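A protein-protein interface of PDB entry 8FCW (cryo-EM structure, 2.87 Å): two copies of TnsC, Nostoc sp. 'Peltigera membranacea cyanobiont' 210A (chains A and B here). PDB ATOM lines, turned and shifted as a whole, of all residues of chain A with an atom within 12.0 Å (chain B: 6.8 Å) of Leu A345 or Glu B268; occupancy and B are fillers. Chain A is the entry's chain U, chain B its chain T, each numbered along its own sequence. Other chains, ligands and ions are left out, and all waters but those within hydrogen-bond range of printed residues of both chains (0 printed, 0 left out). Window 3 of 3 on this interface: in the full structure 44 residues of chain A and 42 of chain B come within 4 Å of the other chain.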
ATOM      1  N   GLU A 333     -18.290 -13.641 -21.975  1.00  0.00           N
ATOM      2  CA  GLU A 333     -18.731 -15.024 -22.006  1.00  0.00           C
ATOM      3  C   GLU A 333     -18.732 -15.527 -23.440  1.00  0.00           C
ATOM      4  O   GLU A 333     -18.446 -16.706 -23.697  1.00  0.00           O
ATOM      5  CB  GLU A 333     -20.111 -15.156 -21.346  1.00  0.00           C
ATOM      6  CG  GLU A 333     -20.634 -16.578 -21.043  1.00  0.00           C
ATOM      7  CD  GLU A 333     -20.948 -17.418 -22.288  1.00  0.00           C
ATOM      8  OE1 GLU A 333     -21.130 -18.645 -22.115  1.00  0.00           O
ATOM      9  OE2 GLU A 333     -21.041 -16.887 -23.425  1.00  0.00           O
ATOM     10  N   ALA A 334     -18.999 -14.637 -24.378  1.00  0.00           N
ATOM     11  CA  ALA A 334     -19.044 -15.010 -25.774  1.00  0.00           C
ATOM     12  C   ALA A 334     -17.706 -15.527 -26.235  1.00  0.00           C
ATOM     13  O   ALA A 334     -17.640 -16.523 -26.946  1.00  0.00           O
ATOM     14  CB  ALA A 334     -19.478 -13.834 -26.630  1.00  0.00           C
ATOM     15  N   ASP A 335     -16.621 -14.876 -25.827  1.00  0.00           N
ATOM     16  CA  ASP A 335     -15.294 -15.310 -26.239  1.00  0.00           C
ATOM     17  C   ASP A 335     -15.011 -16.747 -25.829  1.00  0.00           C
ATOM     18  O   ASP A 335     -14.277 -17.450 -26.515  1.00  0.00           O
ATOM     19  CB  ASP A 335     -14.228 -14.396 -25.648  1.00  0.00           C
ATOM     20  CG  ASP A 335     -14.493 -12.936 -25.906  1.00  0.00           C
ATOM     21  OD1 ASP A 335     -15.073 -12.619 -26.965  1.00  0.00           O
ATOM     22  OD2 ASP A 335     -14.105 -12.114 -25.045  1.00  0.00           O
ATOM     23  N   VAL A 336     -15.573 -17.180 -24.710  1.00  0.00           N
ATOM     24  CA  VAL A 336     -15.453 -18.549 -24.279  1.00  0.00           C
ATOM     25  C   VAL A 336     -16.136 -19.466 -25.281  1.00  0.00           C
ATOM     26  O   VAL A 336     -15.671 -20.575 -25.545  1.00  0.00           O
ATOM     27  CB  VAL A 336     -16.033 -18.734 -22.879  1.00  0.00           C
ATOM     28  CG1 VAL A 336     -15.937 -20.181 -22.424  1.00  0.00           C
ATOM     29  CG2 VAL A 336     -15.323 -17.832 -21.895  1.00  0.00           C
ATOM     30  N   GLN A 337     -17.236 -19.012 -25.858  1.00  0.00           N
ATOM     31  CA  GLN A 337     -18.043 -19.868 -26.712  1.00  0.00           C
ATOM     32  C   GLN A 337     -17.298 -20.221 -27.981  1.00  0.00           C
ATOM     33  O   GLN A 337     -17.304 -21.379 -28.398  1.00  0.00           O
ATOM     34  CB  GLN A 337     -19.366 -19.204 -27.039  1.00  0.00           C
ATOM     35  CG  GLN A 337     -20.495 -20.170 -27.357  1.00  0.00           C
ATOM     36  CD  GLN A 337     -20.448 -21.432 -26.518  1.00  0.00           C
ATOM     37  OE1 GLN A 337     -20.490 -21.377 -25.294  1.00  0.00           O
ATOM     38  NE2 GLN A 337     -20.352 -22.580 -27.178  1.00  0.00           N
ATOM     39  N   ASN A 338     -16.634 -19.251 -28.601  1.00  0.00           N
ATOM     40  CA  ASN A 338     -15.855 -19.551 -29.788  1.00  0.00           C
ATOM     41  C   ASN A 338     -14.694 -20.469 -29.481  1.00  0.00           C
ATOM     42  O   ASN A 338     -14.352 -21.352 -30.283  1.00  0.00           O
ATOM     43  CB  ASN A 338     -15.331 -18.273 -30.428  1.00  0.00           C
ATOM     44  CG  ASN A 338     -16.357 -17.182 -30.450  1.00  0.00           C
ATOM     45  OD1 ASN A 338     -16.837 -16.770 -29.408  1.00  0.00           O
ATOM     46  ND2 ASN A 338     -16.702 -16.705 -31.632  1.00  0.00           N
ATOM     47  N   LEU A 339     -14.082 -20.289 -28.322  1.00  0.00           N
ATOM     48  CA  LEU A 339     -12.986 -21.155 -27.930  1.00  0.00           C
ATOM     49  C   LEU A 339     -13.467 -22.575 -27.772  1.00  0.00           C
ATOM     50  O   LEU A 339     -12.807 -23.512 -28.211  1.00  0.00           O
ATOM     51  CB  LEU A 339     -12.356 -20.654 -26.638  1.00  0.00           C
ATOM     52  CG  LEU A 339     -11.219 -21.456 -26.041  1.00  0.00           C
ATOM     53  CD1 LEU A 339     -10.199 -21.826 -27.094  1.00  0.00           C
ATOM     54  CD2 LEU A 339     -10.553 -20.676 -24.928  1.00  0.00           C
ATOM     55  N   ARG A 340     -14.623 -22.762 -27.155  1.00  0.00           N
ATOM     56  CA  ARG A 340     -15.167 -24.093 -26.993  1.00  0.00           C
ATOM     57  C   ARG A 340     -15.641 -24.647 -28.317  1.00  0.00           C
ATOM     58  O   ARG A 340     -15.497 -25.849 -28.594  1.00  0.00           O
ATOM     59  CB  ARG A 340     -16.293 -24.087 -25.976  1.00  0.00           C
ATOM     60  CG  ARG A 340     -15.866 -23.723 -24.563  1.00  0.00           C
ATOM     61  CD  ARG A 340     -16.242 -24.816 -23.576  1.00  0.00           C
ATOM     62  NE  ARG A 340     -17.601 -25.307 -23.835  1.00  0.00           N
ATOM     63  CZ  ARG A 340     -18.258 -26.161 -23.069  1.00  0.00           C
ATOM     64  NH1 ARG A 340     -17.697 -26.625 -21.967  1.00  0.00           N
ATOM     65  NH2 ARG A 340     -19.485 -26.528 -23.399  1.00  0.00           N
ATOM     66  N   SER A 341     -16.199 -23.796 -29.156  1.00  0.00           N
ATOM     67  CA  SER A 341     -16.686 -24.226 -30.454  1.00  0.00           C
ATOM     68  C   SER A 341     -15.544 -24.684 -31.326  1.00  0.00           C
ATOM     69  O   SER A 341     -15.658 -25.692 -32.027  1.00  0.00           O
ATOM     70  CB  SER A 341     -17.455 -23.100 -31.145  1.00  0.00           C
ATOM     71  OG  SER A 341     -18.569 -22.695 -30.373  1.00  0.00           O
ATOM     72  N   ALA A 342     -14.444 -23.949 -31.311  1.00  0.00           N
ATOM     73  CA  ALA A 342     -13.305 -24.306 -32.134  1.00  0.00           C
ATOM     74  C   ALA A 342     -12.707 -25.620 -31.680  1.00  0.00           C
ATOM     75  O   ALA A 342     -12.299 -26.443 -32.497  1.00  0.00           O
ATOM     76  CB  ALA A 342     -12.265 -23.205 -32.104  1.00  0.00           C
ATOM     77  N   LEU A 343     -12.646 -25.832 -30.374  1.00  0.00           N
ATOM     78  CA  LEU A 343     -12.050 -27.033 -29.825  1.00  0.00           C
ATOM     79  C   LEU A 343     -12.945 -28.244 -29.985  1.00  0.00           C
ATOM     80  O   LEU A 343     -12.460 -29.366 -29.951  1.00  0.00           O
ATOM     81  CB  LEU A 343     -11.711 -26.831 -28.349  1.00  0.00           C
ATOM     82  CG  LEU A 343     -10.496 -25.981 -28.037  1.00  0.00           C
ATOM     83  CD1 LEU A 343     -10.590 -25.466 -26.621  1.00  0.00           C
ATOM     84  CD2 LEU A 343      -9.235 -26.787 -28.196  1.00  0.00           C
ATOM     85  N   GLY A 344     -14.238 -28.038 -30.149  1.00  0.00           N
ATOM     86  CA  GLY A 344     -15.175 -29.133 -30.227  1.00  0.00           C
ATOM     87  C   GLY A 344     -15.835 -29.506 -28.925  1.00  0.00           C
ATOM     88  O   GLY A 344     -16.410 -30.583 -28.827  1.00  0.00           O
ATOM     89  N   LEU A 345     -15.747 -28.646 -27.928  1.00  0.00           N
ATOM     90  CA  LEU A 345     -16.342 -28.900 -26.626  1.00  0.00           C
ATOM     91  C   LEU A 345     -17.754 -28.361 -26.507  1.00  0.00           C
ATOM     92  O   LEU A 345     -18.300 -28.274 -25.414  1.00  0.00           O
ATOM     93  CB  LEU A 345     -15.483 -28.283 -25.527  1.00  0.00           C
ATOM     94  CG  LEU A 345     -14.039 -28.705 -25.432  1.00  0.00           C
ATOM     95  CD1 LEU A 345     -13.270 -27.805 -24.465  1.00  0.00           C
ATOM     96  CD2 LEU A 345     -14.028 -30.128 -24.934  1.00  0.00           C
ATOM     97  N   GLY A 346     -18.374 -28.078 -27.633  1.00  0.00           N
ATOM     98  CA  GLY A 346     -19.707 -27.503 -27.609  1.00  0.00           C
ATOM     99  C   GLY A 346     -20.736 -28.476 -27.083  1.00  0.00           C
ATOM    100  O   GLY A 346     -20.491 -29.681 -27.010  1.00  0.00           O
ATOM    101  N   ALA B 235      -9.919 -33.462 -28.906  1.00  0.00           N
ATOM    102  CA  ALA B 235     -11.239 -33.718 -28.347  1.00  0.00           C
ATOM    103  C   ALA B 235     -12.129 -34.478 -29.310  1.00  0.00           C
ATOM    104  O   ALA B 235     -13.079 -35.128 -28.899  1.00  0.00           O
ATOM    105  CB  ALA B 235     -11.909 -32.427 -27.956  1.00  0.00           C
ATOM    106  N   VAL B 241      -9.921 -38.340 -25.605  1.00  0.00           N
ATOM    107  CA  VAL B 241     -10.731 -37.840 -24.513  1.00  0.00           C
ATOM    108  C   VAL B 241     -10.622 -38.765 -23.320  1.00  0.00           C
ATOM    109  O   VAL B 241     -10.478 -38.310 -22.166  1.00  0.00           O
ATOM    110  CB  VAL B 241     -12.189 -37.660 -24.932  1.00  0.00           C
ATOM    111  CG1 VAL B 241     -13.043 -37.275 -23.724  1.00  0.00           C
ATOM    112  CG2 VAL B 241     -12.281 -36.584 -26.000  1.00  0.00           C
ATOM    113  N   PHE B 244      -7.221 -38.276 -21.722  1.00  0.00           N
ATOM    114  CA  PHE B 244      -7.169 -37.040 -20.960  1.00  0.00           C
ATOM    115  C   PHE B 244      -7.897 -37.200 -19.644  1.00  0.00           C
ATOM    116  O   PHE B 244      -7.442 -36.704 -18.599  1.00  0.00           O
ATOM    117  CB  PHE B 244      -7.745 -35.883 -21.762  1.00  0.00           C
ATOM    118  CG  PHE B 244      -7.502 -34.534 -21.147  1.00  0.00           C
ATOM    119  CD1 PHE B 244      -6.218 -34.081 -20.939  1.00  0.00           C
ATOM    120  CD2 PHE B 244      -8.554 -33.724 -20.770  1.00  0.00           C
ATOM    121  CE1 PHE B 244      -5.988 -32.858 -20.344  1.00  0.00           C
ATOM    122  CE2 PHE B 244      -8.323 -32.504 -20.177  1.00  0.00           C
ATOM    123  CZ  PHE B 244      -7.045 -32.059 -19.983  1.00  0.00           C
ATOM    124  N   LYS B 245      -9.027 -37.887 -19.658  1.00  0.00           N
ATOM    125  CA  LYS B 245      -9.769 -38.120 -18.439  1.00  0.00           C
ATOM    126  C   LYS B 245      -8.993 -39.004 -17.487  1.00  0.00           C
ATOM    127  O   LYS B 245      -9.031 -38.796 -16.271  1.00  0.00           O
ATOM    128  CB  LYS B 245     -11.120 -38.734 -18.740  1.00  0.00           C
ATOM    129  CG  LYS B 245     -12.121 -37.783 -19.368  1.00  0.00           C
ATOM    130  CD  LYS B 245     -13.446 -38.479 -19.603  1.00  0.00           C
ATOM    131  CE  LYS B 245     -14.454 -37.521 -20.193  1.00  0.00           C
ATOM    132  NZ  LYS B 245     -15.759 -38.173 -20.479  1.00  0.00           N
ATOM    133  N   LEU B 248      -6.427 -36.852 -15.853  1.00  0.00           N
ATOM    134  CA  LEU B 248      -7.057 -36.027 -14.847  1.00  0.00           C
ATOM    135  C   LEU B 248      -7.337 -36.848 -13.611  1.00  0.00           C
ATOM    136  O   LEU B 248      -7.157 -36.370 -12.490  1.00  0.00           O
ATOM    137  CB  LEU B 248      -8.335 -35.411 -15.390  1.00  0.00           C
ATOM    138  CG  LEU B 248      -8.275 -33.966 -15.867  1.00  0.00           C
ATOM    139  CD1 LEU B 248      -9.600 -33.561 -16.479  1.00  0.00           C
ATOM    140  CD2 LEU B 248      -7.958 -33.027 -14.710  1.00  0.00           C
ATOM    141  N   LEU B 263     -12.349 -34.030 -10.385  1.00  0.00           N
ATOM    142  CA  LEU B 263     -11.804 -33.300 -11.503  1.00  0.00           C
ATOM    143  C   LEU B 263     -12.293 -33.820 -12.841  1.00  0.00           C
ATOM    144  O   LEU B 263     -12.311 -33.071 -13.795  1.00  0.00           O
ATOM    145  CB  LEU B 263     -10.290 -33.351 -11.451  1.00  0.00           C
ATOM    146  CG  LEU B 263      -9.545 -32.127 -10.952  1.00  0.00           C
ATOM    147  CD1 LEU B 263     -10.212 -31.565  -9.718  1.00  0.00           C
ATOM    148  CD2 LEU B 263      -8.071 -32.417 -10.734  1.00  0.00           C
ATOM    149  N   VAL B 264     -12.693 -35.080 -12.920  1.00  0.00           N
ATOM    150  CA  VAL B 264     -13.183 -35.633 -14.166  1.00  0.00           C
ATOM    151  C   VAL B 264     -14.498 -34.960 -14.548  1.00  0.00           C
ATOM    152  O   VAL B 264     -14.848 -34.884 -15.732  1.00  0.00           O
ATOM    153  CB  VAL B 264     -13.362 -37.148 -14.078  1.00  0.00           C
ATOM    154  CG1 VAL B 264     -13.680 -37.739 -15.444  1.00  0.00           C
ATOM    155  CG2 VAL B 264     -12.108 -37.785 -13.564  1.00  0.00           C
ATOM    156  N   ASP B 265     -15.225 -34.453 -13.564  1.00  0.00           N
ATOM    157  CA  ASP B 265     -16.504 -33.824 -13.846  1.00  0.00           C
ATOM    158  C   ASP B 265     -16.325 -32.608 -14.749  1.00  0.00           C
ATOM    159  O   ASP B 265     -17.006 -32.459 -15.754  1.00  0.00           O
ATOM    160  CB  ASP B 265     -17.197 -33.446 -12.544  1.00  0.00           C
ATOM    161  CG  ASP B 265     -18.620 -32.967 -12.757  1.00  0.00           C
ATOM    162  OD1 ASP B 265     -19.163 -33.185 -13.859  1.00  0.00           O
ATOM    163  OD2 ASP B 265     -19.195 -32.371 -11.821  1.00  0.00           O
ATOM    164  N   HIS B 266     -15.408 -31.728 -14.389  1.00  0.00           N
ATOM    165  CA  HIS B 266     -15.108 -30.559 -15.186  1.00  0.00           C
ATOM    166  C   HIS B 266     -13.954 -30.820 -16.136  1.00  0.00           C
ATOM    167  O   HIS B 266     -12.974 -30.071 -16.186  1.00  0.00           O
ATOM    168  CB  HIS B 266     -14.793 -29.380 -14.276  1.00  0.00           C
ATOM    169  CG  HIS B 266     -15.567 -29.371 -12.998  1.00  0.00           C
ATOM    170  ND1 HIS B 266     -15.198 -30.127 -11.913  1.00  0.00           N
ATOM    171  CD2 HIS B 266     -16.681 -28.698 -12.631  1.00  0.00           C
ATOM    172  CE1 HIS B 266     -16.051 -29.926 -10.928  1.00  0.00           C
ATOM    173  NE2 HIS B 266     -16.963 -29.065 -11.338  1.00  0.00           N
ATOM    174  N   TRP B 267     -14.056 -31.894 -16.902  1.00  0.00           N
ATOM    175  CA  TRP B 267     -13.012 -32.209 -17.859  1.00  0.00           C
ATOM    176  C   TRP B 267     -13.065 -31.283 -19.044  1.00  0.00           C
ATOM    177  O   TRP B 267     -12.039 -30.967 -19.655  1.00  0.00           O
ATOM    178  CB  TRP B 267     -13.103 -33.665 -18.312  1.00  0.00           C
ATOM    179  CG  TRP B 267     -14.250 -33.971 -19.186  1.00  0.00           C
ATOM    180  CD1 TRP B 267     -15.509 -34.299 -18.793  1.00  0.00           C
ATOM    181  CD2 TRP B 267     -14.261 -33.973 -20.616  1.00  0.00           C
ATOM    182  NE1 TRP B 267     -16.311 -34.497 -19.890  1.00  0.00           N
ATOM    183  CE2 TRP B 267     -15.564 -34.303 -21.022  1.00  0.00           C
ATOM    184  CE3 TRP B 267     -13.294 -33.724 -21.593  1.00  0.00           C
ATOM    185  CZ2 TRP B 267     -15.927 -34.387 -22.363  1.00  0.00           C
ATOM    186  CZ3 TRP B 267     -13.649 -33.822 -22.912  1.00  0.00           C
ATOM    187  CH2 TRP B 267     -14.959 -34.128 -23.289  1.00  0.00           C
ATOM    188  N   GLU B 268     -14.254 -30.824 -19.378  1.00  0.00           N
ATOM    189  CA  GLU B 268     -14.413 -29.885 -20.466  1.00  0.00           C
ATOM    190  C   GLU B 268     -13.701 -28.588 -20.171  1.00  0.00           C
ATOM    191  O   GLU B 268     -13.057 -28.014 -21.065  1.00  0.00           O
ATOM    192  CB  GLU B 268     -15.896 -29.651 -20.749  1.00  0.00           C
ATOM    193  CG  GLU B 268     -16.658 -30.920 -21.118  1.00  0.00           C
ATOM    194  CD  GLU B 268     -17.752 -30.700 -22.127  1.00  0.00           C
ATOM    195  OE1 GLU B 268     -17.774 -29.618 -22.724  1.00  0.00           O
ATOM    196  OE2 GLU B 268     -18.576 -31.609 -22.338  1.00  0.00           O
ATOM    197  N   TYR B 269     -13.786 -28.117 -18.939  1.00  0.00           N
ATOM    198  CA  TYR B 269     -13.149 -26.849 -18.583  1.00  0.00           C
ATOM    199  C   TYR B 269     -11.651 -27.006 -18.650  1.00  0.00           C
ATOM    200  O   TYR B 269     -10.933 -26.121 -19.124  1.00  0.00           O
ATOM    201  CB  TYR B 269     -13.584 -26.398 -17.191  1.00  0.00           C
ATOM    202  CG  TYR B 269     -13.014 -25.082 -16.731  1.00  0.00           C
ATOM    203  CD1 TYR B 269     -13.085 -23.957 -17.530  1.00  0.00           C
ATOM    204  CD2 TYR B 269     -12.405 -24.966 -15.493  1.00  0.00           C
ATOM    205  CE1 TYR B 269     -12.557 -22.751 -17.108  1.00  0.00           C
ATOM    206  CE2 TYR B 269     -11.878 -23.764 -15.066  1.00  0.00           C
ATOM    207  CZ  TYR B 269     -11.951 -22.661 -15.882  1.00  0.00           C
ATOM    208  OH  TYR B 269     -11.421 -21.461 -15.471  1.00  0.00           O
ATOM    209  N   PHE B 270     -11.147 -28.135 -18.176  1.00  0.00           N
ATOM    210  CA  PHE B 270      -9.723 -28.391 -18.197  1.00  0.00           C
ATOM    211  C   PHE B 270      -9.224 -28.437 -19.627  1.00  0.00           C
ATOM    212  O   PHE B 270      -8.161 -27.903 -19.929  1.00  0.00           O
ATOM    213  CB  PHE B 270      -9.423 -29.686 -17.474  1.00  0.00           C
ATOM    214  CG  PHE B 270      -9.216 -29.528 -16.001  1.00  0.00           C
ATOM    215  CD1 PHE B 270      -8.104 -28.870 -15.516  1.00  0.00           C
ATOM    216  CD2 PHE B 270     -10.118 -30.050 -15.103  1.00  0.00           C
ATOM    217  CE1 PHE B 270      -7.901 -28.722 -14.165  1.00  0.00           C
ATOM    218  CE2 PHE B 270      -9.918 -29.905 -13.750  1.00  0.00           C
ATOM    219  CZ  PHE B 270      -8.807 -29.239 -13.280  1.00  0.00           C
ATOM    220  N   TYR B 271      -9.974 -29.058 -20.518  1.00  0.00           N
ATOM    221  CA  TYR B 271      -9.578 -29.129 -21.914  1.00  0.00           C
ATOM    222  C   TYR B 271      -9.595 -27.765 -22.522  1.00  0.00           C
ATOM    223  O   TYR B 271      -8.700 -27.408 -23.309  1.00  0.00           O
ATOM    224  CB  TYR B 271     -10.473 -30.066 -22.694  1.00  0.00           C
ATOM    225  CG  TYR B 271      -9.975 -30.394 -24.073  1.00  0.00           C
ATOM    226  CD1 TYR B 271      -9.141 -31.462 -24.304  1.00  0.00           C
ATOM    227  CD2 TYR B 271     -10.351 -29.623 -25.145  1.00  0.00           C
ATOM    228  CE1 TYR B 271      -8.698 -31.743 -25.582  1.00  0.00           C
ATOM    229  CE2 TYR B 271      -9.921 -29.904 -26.417  1.00  0.00           C
ATOM    230  CZ  TYR B 271      -9.093 -30.956 -26.633  1.00  0.00           C
ATOM    231  OH  TYR B 271      -8.667 -31.208 -27.911  1.00  0.00           O
ATOM    232  N   GLU B 272     -10.581 -26.962 -22.171  1.00  0.00           N
ATOM    233  CA  GLU B 272     -10.712 -25.639 -22.743  1.00  0.00           C
ATOM    234  C   GLU B 272      -9.529 -24.780 -22.356  1.00  0.00           C
ATOM    235  O   GLU B 272      -9.000 -24.015 -23.161  1.00  0.00           O
ATOM    236  CB  GLU B 272     -12.013 -25.006 -22.291  1.00  0.00           C
ATOM    237  CG  GLU B 272     -12.153 -23.532 -22.605  1.00  0.00           C
ATOM    238  CD  GLU B 272     -13.056 -22.816 -21.626  1.00  0.00           C
ATOM    239  OE1 GLU B 272     -14.140 -23.362 -21.308  1.00  0.00           O
ATOM    240  OE2 GLU B 272     -12.663 -21.707 -21.167  1.00  0.00           O
ATOM    241  N   ARG B 273      -9.077 -24.900 -21.121  1.00  0.00           N
ATOM    242  CA  ARG B 273      -8.024 -24.039 -20.612  1.00  0.00           C
ATOM    243  C   ARG B 273      -6.645 -24.669 -20.685  1.00  0.00           C
ATOM    244  O   ARG B 273      -5.671 -24.062 -20.215  1.00  0.00           O
ATOM    245  CB  ARG B 273      -8.312 -23.650 -19.173  1.00  0.00           C
ATOM    246  CG  ARG B 273      -9.634 -22.947 -18.987  1.00  0.00           C
ATOM    247  CD  ARG B 273      -9.599 -21.596 -19.653  1.00  0.00           C
ATOM    248  NE  ARG B 273     -10.753 -20.828 -19.260  1.00  0.00           N
ATOM    249  CZ  ARG B 273     -10.891 -19.537 -19.412  1.00  0.00           C
ATOM    250  NH1 ARG B 273      -9.954 -18.841 -19.998  1.00  0.00           N
ATOM    251  NH2 ARG B 273     -11.992 -18.975 -18.992  1.00  0.00           N
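OE1 of Glu B268 sits close to O of Leu A345, 3.1 Å away. The side-chain carboxylate (OE1) of Glu B268 lies within salt-bridge range of the guanidinium group (NH1) of Arg A340, at 3.1 Å.
N of Ala B235 sits at hydrogen-bond distance from OH of Tyr B271 (2.8 Å). The side-chain carboxylate of Glu B272 lies within salt-bridge range of the guanidinium group of Arg B273, 2.8 Å away. O of Arg A340 lies within hydrogen-bond range of N of Leu A345, 2.9 Å away.
Among the printed residues, pairs that only touch across the chains: Arg A340 with Glu B272 (3.4 Å), Leu A345 with Tyr B271 (3.5 Å), Leu A345 with Glu B272 (3.6 Å), Leu A343 with Tyr B271 (3.7 Å), Leu A343 with Ala B235 (3.7 Å), Val A336 with Glu B272 (3.8 Å) and Leu A343 with Glu B272 (3.9 Å).
Leu A345 touches just these residues of chain B: Glu B268 (3.1 Å), Tyr B271 (3.5 Å) and Glu B272 (3.6 Å). Of chain A, only Arg A340 (3.1 Å) and Leu A345 (3.1 Å) come within 4 Å of Glu B268. Of chain A, only Leu A343 (3.7 Å) comes within 4 Å of Ala B235. Of the printed residues of chain B, Leu A343 touches Ala B235 (3.7 Å), Tyr B271 (3.7 Å) and Glu B272 (3.9 Å). Of the printed residues of chain B, Val A336 touches Glu B272. Printed residues of chain A within 4 Å of Glu B272: Val A336 (3.8 Å), Arg A340 (3.4 Å), Leu A343 (3.9 Å) and Leu A345 (3.6 Å). Of the printed residues of chain B, Arg A340 touches Glu B268 and Glu B272. Ser A341 touches none of the printed residues of chain B. The nearest residue of chain A that does not touch Glu B268 is Gly A346 (5.1 Å). The nearest printed residue of chain B that does not touch Val A336 is Arg B273 (4.6 Å).
Hydrophobic or aromatic side chains of chain B within 4 Å of the printed part of chain A: Ala B235 and Tyr B271. Printed residues of chain A that touch a printed residue of chain B: Val A336, Arg A340, Leu A343 and Leu A345. Hydrophobic or aromatic side chains of chain A that line the printed part of chain B: Val A336, Leu A343 and Leu A345. Among the printed residues, 9 pairs touch across the chains. Among the printed residues, Asp or Glu carboxylates within 4 Å of a Lys or Arg side-chain nitrogen of the other chain: Arg A340 with Glu B268.
No position is printed for both chains.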
